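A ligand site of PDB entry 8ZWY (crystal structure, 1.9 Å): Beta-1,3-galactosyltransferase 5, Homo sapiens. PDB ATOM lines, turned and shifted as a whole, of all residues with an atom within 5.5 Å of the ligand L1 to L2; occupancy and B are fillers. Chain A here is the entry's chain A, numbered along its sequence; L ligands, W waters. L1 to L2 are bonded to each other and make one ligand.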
ATOM      1  N   TYR A  98      11.391 -26.419  27.955  1.00  0.00           N
ATOM      2  CA  TYR A  98      10.384 -26.276  26.863  1.00  0.00           C
ATOM      3  C   TYR A  98      10.987 -26.711  25.508  1.00  0.00           C
ATOM      4  O   TYR A  98      10.337 -27.503  24.840  1.00  0.00           O
ATOM      5  CB  TYR A  98       9.758 -24.883  26.789  1.00  0.00           C
ATOM      6  CG  TYR A  98       8.466 -24.874  25.970  1.00  0.00           C
ATOM      7  CD1 TYR A  98       7.239 -25.131  26.557  1.00  0.00           C
ATOM      8  CD2 TYR A  98       8.502 -24.632  24.607  1.00  0.00           C
ATOM      9  CE1 TYR A  98       6.077 -25.129  25.806  1.00  0.00           C
ATOM     10  CE2 TYR A  98       7.342 -24.631  23.842  1.00  0.00           C
ATOM     11  CZ  TYR A  98       6.125 -24.894  24.446  1.00  0.00           C
ATOM     12  OH  TYR A  98       5.000 -24.889  23.687  1.00  0.00           O
ATOM     13  N   LYS A 155      -4.332 -29.312  12.556  1.00  0.00           N
ATOM     14  CA  LYS A 155      -3.709 -28.045  12.091  1.00  0.00           C
ATOM     15  C   LYS A 155      -3.124 -28.365  10.699  1.00  0.00           C
ATOM     16  O   LYS A 155      -2.011 -28.908  10.633  1.00  0.00           O
ATOM     17  CB  LYS A 155      -2.755 -27.521  13.168  1.00  0.00           C
ATOM     18  CG  LYS A 155      -3.301 -27.316  14.572  1.00  0.00           C
ATOM     19  CD  LYS A 155      -2.222 -27.003  15.592  1.00  0.00           C
ATOM     20  CE  LYS A 155      -1.585 -25.662  15.419  1.00  0.00           C
ATOM     21  NZ  LYS A 155      -2.520 -24.563  15.639  1.00  0.00           N
ATOM     22  N   GLU A 158      -0.463 -24.840   8.301  1.00  0.00           N
ATOM     23  CA  GLU A 158       0.292 -24.016   9.266  1.00  0.00           C
ATOM     24  C   GLU A 158       1.569 -23.441   8.647  1.00  0.00           C
ATOM     25  O   GLU A 158       2.195 -24.096   7.804  1.00  0.00           O
ATOM     26  CB  GLU A 158       0.561 -24.816  10.549  1.00  0.00           C
ATOM     27  CG  GLU A 158      -0.699 -25.227  11.284  1.00  0.00           C
ATOM     28  CD  GLU A 158      -1.223 -23.996  11.983  1.00  0.00           C
ATOM     29  OE1 GLU A 158      -0.383 -23.153  12.296  1.00  0.00           O
ATOM     30  OE2 GLU A 158      -2.427 -23.851  12.198  1.00  0.00           O
ATOM     31  N   PHE A 159       1.906 -22.236   9.077  1.00  0.00           N
ATOM     32  CA  PHE A 159       3.159 -21.600   8.635  1.00  0.00           C
ATOM     33  C   PHE A 159       4.053 -21.470   9.844  1.00  0.00           C
ATOM     34  O   PHE A 159       3.589 -21.151  10.940  1.00  0.00           O
ATOM     35  CB  PHE A 159       2.777 -20.282   7.956  1.00  0.00           C
ATOM     36  CG  PHE A 159       1.850 -20.474   6.769  1.00  0.00           C
ATOM     37  CD1 PHE A 159       2.339 -20.842   5.524  1.00  0.00           C
ATOM     38  CD2 PHE A 159       0.474 -20.310   6.909  1.00  0.00           C
ATOM     39  CE1 PHE A 159       1.486 -21.031   4.451  1.00  0.00           C
ATOM     40  CE2 PHE A 159      -0.376 -20.512   5.831  1.00  0.00           C
ATOM     41  CZ  PHE A 159       0.132 -20.880   4.611  1.00  0.00           C
ATOM     42  N   PRO A 160       5.359 -21.743   9.696  1.00  0.00           N
ATOM     43  CA  PRO A 160       6.268 -21.506  10.788  1.00  0.00           C
ATOM     44  C   PRO A 160       6.142 -20.043  11.266  1.00  0.00           C
ATOM     45  O   PRO A 160       5.901 -19.141  10.454  1.00  0.00           O
ATOM     46  CB  PRO A 160       7.668 -21.800  10.233  1.00  0.00           C
ATOM     47  CG  PRO A 160       7.456 -21.993   8.749  1.00  0.00           C
ATOM     48  CD  PRO A 160       5.982 -22.270   8.514  1.00  0.00           C
ATOM     49  N   ILE A 161       6.304 -19.856  12.561  1.00  0.00           N
ATOM     50  CA  ILE A 161       6.259 -18.499  13.174  1.00  0.00           C
ATOM     51  C   ILE A 161       7.673 -17.910  13.127  1.00  0.00           C
ATOM     52  O   ILE A 161       8.575 -18.456  13.752  1.00  0.00           O
ATOM     53  CB  ILE A 161       5.707 -18.579  14.607  1.00  0.00           C
ATOM     54  CG1 ILE A 161       4.224 -18.966  14.628  1.00  0.00           C
ATOM     55  CG2 ILE A 161       5.965 -17.282  15.375  1.00  0.00           C
ATOM     56  CD1 ILE A 161       3.709 -19.369  15.994  1.00  0.00           C
ATOM     57  N   TRP A 168       6.922 -19.920  20.004  1.00  0.00           N
ATOM     58  CA  TRP A 168       7.010 -20.968  18.955  1.00  0.00           C
ATOM     59  C   TRP A 168       7.881 -20.506  17.776  1.00  0.00           C
ATOM     60  O   TRP A 168       7.828 -21.102  16.703  1.00  0.00           O
ATOM     61  CB  TRP A 168       5.596 -21.350  18.532  1.00  0.00           C
ATOM     62  CG  TRP A 168       4.762 -21.881  19.667  1.00  0.00           C
ATOM     63  CD1 TRP A 168       5.088 -22.866  20.546  1.00  0.00           C
ATOM     64  CD2 TRP A 168       3.437 -21.433  20.038  1.00  0.00           C
ATOM     65  NE1 TRP A 168       4.072 -23.048  21.445  1.00  0.00           N
ATOM     66  CE2 TRP A 168       3.043 -22.196  21.147  1.00  0.00           C
ATOM     67  CE3 TRP A 168       2.562 -20.464  19.524  1.00  0.00           C
ATOM     68  CZ2 TRP A 168       1.815 -22.025  21.767  1.00  0.00           C
ATOM     69  CZ3 TRP A 168       1.348 -20.300  20.134  1.00  0.00           C
ATOM     70  CH2 TRP A 168       0.974 -21.074  21.240  1.00  0.00           C
ATOM     71  N   TYR A 180       4.350 -25.894   7.286  1.00  0.00           N
ATOM     72  CA  TYR A 180       4.549 -27.106   8.080  1.00  0.00           C
ATOM     73  C   TYR A 180       3.710 -28.228   7.471  1.00  0.00           C
ATOM     74  O   TYR A 180       2.746 -27.958   6.756  1.00  0.00           O
ATOM     75  CB  TYR A 180       4.064 -26.844   9.503  1.00  0.00           C
ATOM     76  CG  TYR A 180       5.006 -26.117  10.462  1.00  0.00           C
ATOM     77  CD1 TYR A 180       6.384 -26.293  10.389  1.00  0.00           C
ATOM     78  CD2 TYR A 180       4.510 -25.259  11.429  1.00  0.00           C
ATOM     79  CE1 TYR A 180       7.242 -25.645  11.261  1.00  0.00           C
ATOM     80  CE2 TYR A 180       5.349 -24.600  12.305  1.00  0.00           C
ATOM     81  CZ  TYR A 180       6.719 -24.795  12.218  1.00  0.00           C
ATOM     82  OH  TYR A 180       7.565 -24.163  13.068  1.00  0.00           O
ATOM     83  N   PHE A 183      -0.355 -31.431  11.164  1.00  0.00           N
ATOM     84  CA  PHE A 183      -0.054 -31.926  12.528  1.00  0.00           C
ATOM     85  C   PHE A 183      -1.252 -31.621  13.450  1.00  0.00           C
ATOM     86  O   PHE A 183      -2.127 -30.870  13.032  1.00  0.00           O
ATOM     87  CB  PHE A 183       1.274 -31.355  13.002  1.00  0.00           C
ATOM     88  CG  PHE A 183       1.294 -29.874  13.332  1.00  0.00           C
ATOM     89  CD1 PHE A 183       1.548 -28.925  12.351  1.00  0.00           C
ATOM     90  CD2 PHE A 183       1.088 -29.427  14.634  1.00  0.00           C
ATOM     91  CE1 PHE A 183       1.590 -27.573  12.662  1.00  0.00           C
ATOM     92  CE2 PHE A 183       1.121 -28.081  14.936  1.00  0.00           C
ATOM     93  CZ  PHE A 183       1.367 -27.162  13.950  1.00  0.00           C
ATOM     94  N   SER A 185      -2.552 -30.231  17.460  1.00  0.00           N
ATOM     95  CA  SER A 185      -2.081 -29.461  18.640  1.00  0.00           C
ATOM     96  C   SER A 185      -1.398 -30.399  19.644  1.00  0.00           C
ATOM     97  O   SER A 185      -2.008 -31.397  20.009  1.00  0.00           O
ATOM     98  CB  SER A 185      -3.170 -28.629  19.338  1.00  0.00           C
ATOM     99  OG  SER A 185      -2.707 -28.086  20.555  1.00  0.00           O
ATOM    100  N   GLY A 186      -0.213 -30.034  20.107  1.00  0.00           N
ATOM    101  CA  GLY A 186       0.461 -30.828  21.151  1.00  0.00           C
ATOM    102  C   GLY A 186      -0.261 -30.776  22.497  1.00  0.00           C
ATOM    103  O   GLY A 186       0.119 -31.514  23.402  1.00  0.00           O
ATOM    104  N   THR A 187      -1.285 -29.925  22.626  1.00  0.00           N
ATOM    105  CA  THR A 187      -2.076 -29.890  23.874  1.00  0.00           C
ATOM    106  C   THR A 187      -2.642 -31.261  24.201  1.00  0.00           C
ATOM    107  O   THR A 187      -2.761 -31.594  25.378  1.00  0.00           O
ATOM    108  CB  THR A 187      -3.195 -28.847  23.749  1.00  0.00           C
ATOM    109  OG1 THR A 187      -4.009 -29.082  22.616  1.00  0.00           O
ATOM    110  CG2 THR A 187      -2.627 -27.430  23.700  1.00  0.00           C
ATOM    111  N   LEU A 211       9.799 -28.178  18.126  1.00  0.00           N
ATOM    112  CA  LEU A 211       8.341 -28.186  18.399  1.00  0.00           C
ATOM    113  C   LEU A 211       7.840 -29.642  18.255  1.00  0.00           C
ATOM    114  O   LEU A 211       7.780 -30.119  17.118  1.00  0.00           O
ATOM    115  CB  LEU A 211       7.625 -27.182  17.520  1.00  0.00           C
ATOM    116  CG  LEU A 211       8.134 -25.743  17.595  1.00  0.00           C
ATOM    117  CD1 LEU A 211       7.416 -24.819  16.630  1.00  0.00           C
ATOM    118  CD2 LEU A 211       8.087 -25.191  19.008  1.00  0.00           C
ATOM    119  N   ASP A 213       4.905 -31.371  18.432  1.00  0.00           N
ATOM    120  CA  ASP A 213       3.718 -31.689  17.603  1.00  0.00           C
ATOM    121  C   ASP A 213       4.081 -31.626  16.115  1.00  0.00           C
ATOM    122  O   ASP A 213       3.652 -32.477  15.363  1.00  0.00           O
ATOM    123  CB  ASP A 213       2.512 -30.848  18.011  1.00  0.00           C
ATOM    124  CG  ASP A 213       2.713 -29.346  18.161  1.00  0.00           C
ATOM    125  OD1 ASP A 213       3.831 -28.850  17.977  1.00  0.00           O
ATOM    126  OD2 ASP A 213       1.711 -28.670  18.436  1.00  0.00           O
ATOM    127  N   VAL A 214       4.863 -30.624  15.737  1.00  0.00           N
ATOM    128  CA  VAL A 214       5.341 -30.489  14.327  1.00  0.00           C
ATOM    129  C   VAL A 214       6.275 -31.681  13.994  1.00  0.00           C
ATOM    130  O   VAL A 214       6.118 -32.263  12.938  1.00  0.00           O
ATOM    131  CB  VAL A 214       6.006 -29.130  14.049  1.00  0.00           C
ATOM    132  CG1 VAL A 214       6.438 -28.991  12.595  1.00  0.00           C
ATOM    133  CG2 VAL A 214       5.109 -27.971  14.457  1.00  0.00           C
ATOM    134  N   PRO A 238      -7.829 -26.597  21.996  1.00  0.00           N
ATOM    135  CA  PRO A 238      -6.591 -25.939  22.394  1.00  0.00           C
ATOM    136  C   PRO A 238      -6.828 -24.493  22.904  1.00  0.00           C
ATOM    137  O   PRO A 238      -6.075 -24.027  23.741  1.00  0.00           O
ATOM    138  CB  PRO A 238      -5.752 -26.002  21.121  1.00  0.00           C
ATOM    139  CG  PRO A 238      -6.312 -27.183  20.359  1.00  0.00           C
ATOM    140  CD  PRO A 238      -7.809 -27.110  20.645  1.00  0.00           C
ATOM    141  N   HIS A 255      -8.055 -27.067  27.012  1.00  0.00           N
ATOM    142  CA  HIS A 255      -6.771 -26.528  27.488  1.00  0.00           C
ATOM    143  C   HIS A 255      -7.009 -25.346  28.439  1.00  0.00           C
ATOM    144  O   HIS A 255      -8.168 -25.030  28.710  1.00  0.00           O
ATOM    145  CB  HIS A 255      -5.981 -26.134  26.238  1.00  0.00           C
ATOM    146  CG  HIS A 255      -4.616 -25.643  26.402  1.00  0.00           C
ATOM    147  ND1 HIS A 255      -4.206 -24.542  25.693  1.00  0.00           N
ATOM    148  CD2 HIS A 255      -3.586 -26.044  27.121  1.00  0.00           C
ATOM    149  CE1 HIS A 255      -2.951 -24.287  25.985  1.00  0.00           C
ATOM    150  NE2 HIS A 255      -2.570 -25.189  26.837  1.00  0.00           N
HETATM  151  C1  LIG L   1      -1.920 -19.634  17.148  1.00  0.00           C
HETATM  152  C2  LIG L   1      -1.750 -21.084  17.594  1.00  0.00           C
HETATM  153  C3  LIG L   1      -0.449 -21.669  17.060  1.00  0.00           C
HETATM  154  C4  LIG L   1      -0.327 -21.431  15.575  1.00  0.00           C
HETATM  155  C5  LIG L   1      -0.436 -19.946  15.310  1.00  0.00           C
HETATM  156  C6  LIG L   1      -0.317 -19.590  13.841  1.00  0.00           C
HETATM  157  C7  LIG L   1      -3.426 -17.844  17.343  1.00  0.00           C
HETATM  158  O1  LIG L   1      -3.205 -19.233  17.517  1.00  0.00           O
HETATM  159  O2  LIG L   1      -1.774 -21.183  19.009  1.00  0.00           O
HETATM  160  O3  LIG L   1      -0.389 -23.056  17.349  1.00  0.00           O
HETATM  161  O4  LIG L   1      -1.365 -22.113  14.913  1.00  0.00           O
HETATM  162  O5  LIG L   1      -1.728 -19.494  15.759  1.00  0.00           O
HETATM  163  O6  LIG L   1      -0.419 -18.202  13.624  1.00  0.00           O
HETATM  164  C1  LG2 L   2       0.874 -23.477  17.751  1.00  0.00           C
HETATM  165  C2  LG2 L   2       0.732 -24.699  18.651  1.00  0.00           C
HETATM  166  C3  LG2 L   2       2.116 -25.225  19.021  1.00  0.00           C
HETATM  167  C4  LG2 L   2       2.905 -25.502  17.755  1.00  0.00           C
HETATM  168  C5  LG2 L   2       3.002 -24.184  16.996  1.00  0.00           C
HETATM  169  C6  LG2 L   2       3.807 -24.262  15.726  1.00  0.00           C
HETATM  170  C7  LG2 L   2      -1.249 -24.863  20.090  1.00  0.00           C
HETATM  171  C8  LG2 L   2      -2.028 -24.176  21.162  1.00  0.00           C
HETATM  172  N1  LG2 L   2      -0.037 -24.377  19.837  1.00  0.00           N
HETATM  173  O1  LG2 L   2       2.010 -26.376  19.841  1.00  0.00           O
HETATM  174  O2  LG2 L   2       4.201 -25.977  18.097  1.00  0.00           O
HETATM  175  O3  LG2 L   2       1.678 -23.785  16.621  1.00  0.00           O
HETATM  176  O4  LG2 L   2       3.844 -22.989  15.105  1.00  0.00           O
HETATM  177  O5  LG2 L   2      -1.703 -25.815  19.474  1.00  0.00           O
HETATM  178  N1  LG3 L   3       6.429 -28.862  30.062  1.00  0.00           N
HETATM  179  C1  LG3 L   3       7.361 -29.854  30.429  1.00  0.00           C
HETATM  180  N2  LG3 L   3       8.617 -29.392  30.729  1.00  0.00           N
HETATM  181  C2  LG3 L   3       9.051 -28.083  30.696  1.00  0.00           C
HETATM  182  C3  LG3 L   3       8.054 -27.123  30.284  1.00  0.00           C
HETATM  183  C4  LG3 L   3       6.794 -27.536  30.014  1.00  0.00           C
HETATM  184  O1  LG3 L   3       7.079 -31.043  30.535  1.00  0.00           O
HETATM  185  O2  LG3 L   3      10.226 -27.828  30.974  1.00  0.00           O
HETATM  186  C5  LG3 L   3       5.055 -29.279  29.773  1.00  0.00           C
HETATM  187  C6  LG3 L   3       3.982 -28.480  30.498  1.00  0.00           C
HETATM  188  O3  LG3 L   3       3.772 -28.956  31.812  1.00  0.00           O
HETATM  189  C7  LG3 L   3       2.784 -28.746  29.596  1.00  0.00           C
HETATM  190  C8  LG3 L   3       3.437 -28.689  28.205  1.00  0.00           C
HETATM  191  O4  LG3 L   3       4.829 -29.023  28.419  1.00  0.00           O
HETATM  192  O5  LG3 L   3       2.225 -30.016  29.892  1.00  0.00           O
HETATM  193  C9  LG3 L   3       3.362 -27.363  27.486  1.00  0.00           C
HETATM  194  O6  LG3 L   3       3.740 -26.343  28.442  1.00  0.00           O
HETATM  195  P1  LG3 L   3       2.840 -25.067  28.664  1.00  0.00           P
HETATM  196  O7  LG3 L   3       3.490 -24.251  29.697  1.00  0.00           O
HETATM  197  O8  LG3 L   3       1.408 -25.461  28.975  1.00  0.00           O
HETATM  198  O9  LG3 L   3       2.815 -24.328  27.294  1.00  0.00           O
HETATM  199  P2  LG3 L   3       1.767 -24.288  26.097  1.00  0.00           P
HETATM  200  O10 LG3 L   3       0.164 -24.697  26.596  1.00  0.00           O
HETATM  201  O11 LG3 L   3       2.477 -25.166  25.026  1.00  0.00           O
HETATM  202  O12 LG3 L   3       1.930 -22.880  25.557  1.00  0.00           O
HETATM  203  O   HOH W   1      -4.092 -25.228  17.912  1.00  0.00           O
HETATM  204  O   HOH W   2      -4.440 -21.922  19.620  1.00  0.00           O
HETATM  205  O   HOH W   3       1.566 -18.413  11.092  1.00  0.00           O
HETATM  206  O   HOH W   4       6.393 -22.148  14.426  1.00  0.00           O
HETATM  207  O   HOH W   5      -4.164 -20.441  14.512  1.00  0.00           O
HETATM  208  O   HOH W   6       4.403 -26.839  21.166  1.00  0.00           O
HETATM  209  O   HOH W   7      -0.074 -24.231  23.621  1.00  0.00           O
HETATM  210  O   HOH W   8      -2.126 -19.090  20.513  1.00  0.00           O
HETATM  211  O   HOH W   9      -0.062 -20.787  10.641  1.00  0.00           O
HETATM  212  O   HOH W  10       0.625 -16.490  15.731  1.00  0.00           O
HETATM  213  O   HOH W  11       0.353 -27.085  21.981  1.00  0.00           O
HETATM  214  O   HOH W  12       2.003 -22.318  12.759  1.00  0.00           O
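O1 of LG2 L2 is in hydrogen-bond range of OD2 of Asp 213, at 2.7 Å. The side-chain hydroxyl (OG) of Ser 185 is in hydrogen-bond range of an oxygen (O5) of LG2 L2 (2.7 Å). An oxygen (O4) of LIG L1 is in hydrogen-bond range of the side-chain amino group of Lys 155, 2.8 Å away. An oxygen (O4) of LIG L1 is in hydrogen-bond range of the side-chain carboxylate (OE1) of Glu 158 (3.0 Å). OH of Tyr 98 lies within hydrogen-bond range of O11 of LG3 L3.
The backbone NH (N) of Gly 186 is in hydrogen-bond range of the side-chain carboxylate (OD2) of Asp 213, at 2.9 Å. The side-chain hydroxyl of Ser 185 lies within hydrogen-bond range of the side-chain hydroxyl of Thr 187, at 2.6 Å. The side-chain carboxylate (OE2) of Glu 158 lies within salt-bridge range of the side-chain amino group (NZ) of Lys 155 (3.5 Å). The backbone NH of Lys 155 is in hydrogen-bond range of the backbone carbonyl oxygen of Phe 183, 2.7 Å away. The backbone carbonyl oxygen (O) of Glu 158 lies within hydrogen-bond range of the backbone NH (N) of Tyr 180, 2.9 Å away. The indole nitrogen (NE1) of Trp 168 lies within hydrogen-bond range of the side-chain hydroxyl (OH) of Tyr 98 (3.0 Å).
CD1 of Ile 161 touches O4 of LG2 L2 (3.7 Å). Trp 168 touches the ligand L1 to L2. CE2 of Tyr 180 touches O4 of LG2 L2, 3.6 Å away. CB of Leu 211 touches O2 of LG2 L2 (3.7 Å). Eight residues have an atom within 4 Å of the ligand L1 to L2: Lys 155, Glu 158, Ile 161, Trp 168, Tyr 180, Ser 185, Leu 211 and Asp 213.
Water W4 lies within hydrogen-bond range of OH of Tyr 180 (2.7 Å), O4 of LG2 L2 (2.8 Å), O of Trp 168 (2.9 Å) and N of Ile 161 (3.0 Å). Water W6 lies within hydrogen-bond range of O1 of LG2 L2 (2.8 Å) and OH of Tyr 98 (3.2 Å). Water W11 lies within hydrogen-bond range of O1 of LG2 L2 and N of Thr 187. Water W1 bridges the side-chain amino group (NZ) of Lys 155 (2.8 Å) and an oxygen (O5) of LG2 L2 (2.9 Å). Water W12 lies within hydrogen-bond range of OE1 of Glu 158, O of Phe 159 and O4 of LG2 L2. Water W3 bridges an oxygen (O6) of LIG L1 and the backbone carbonyl oxygen of Phe 159.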
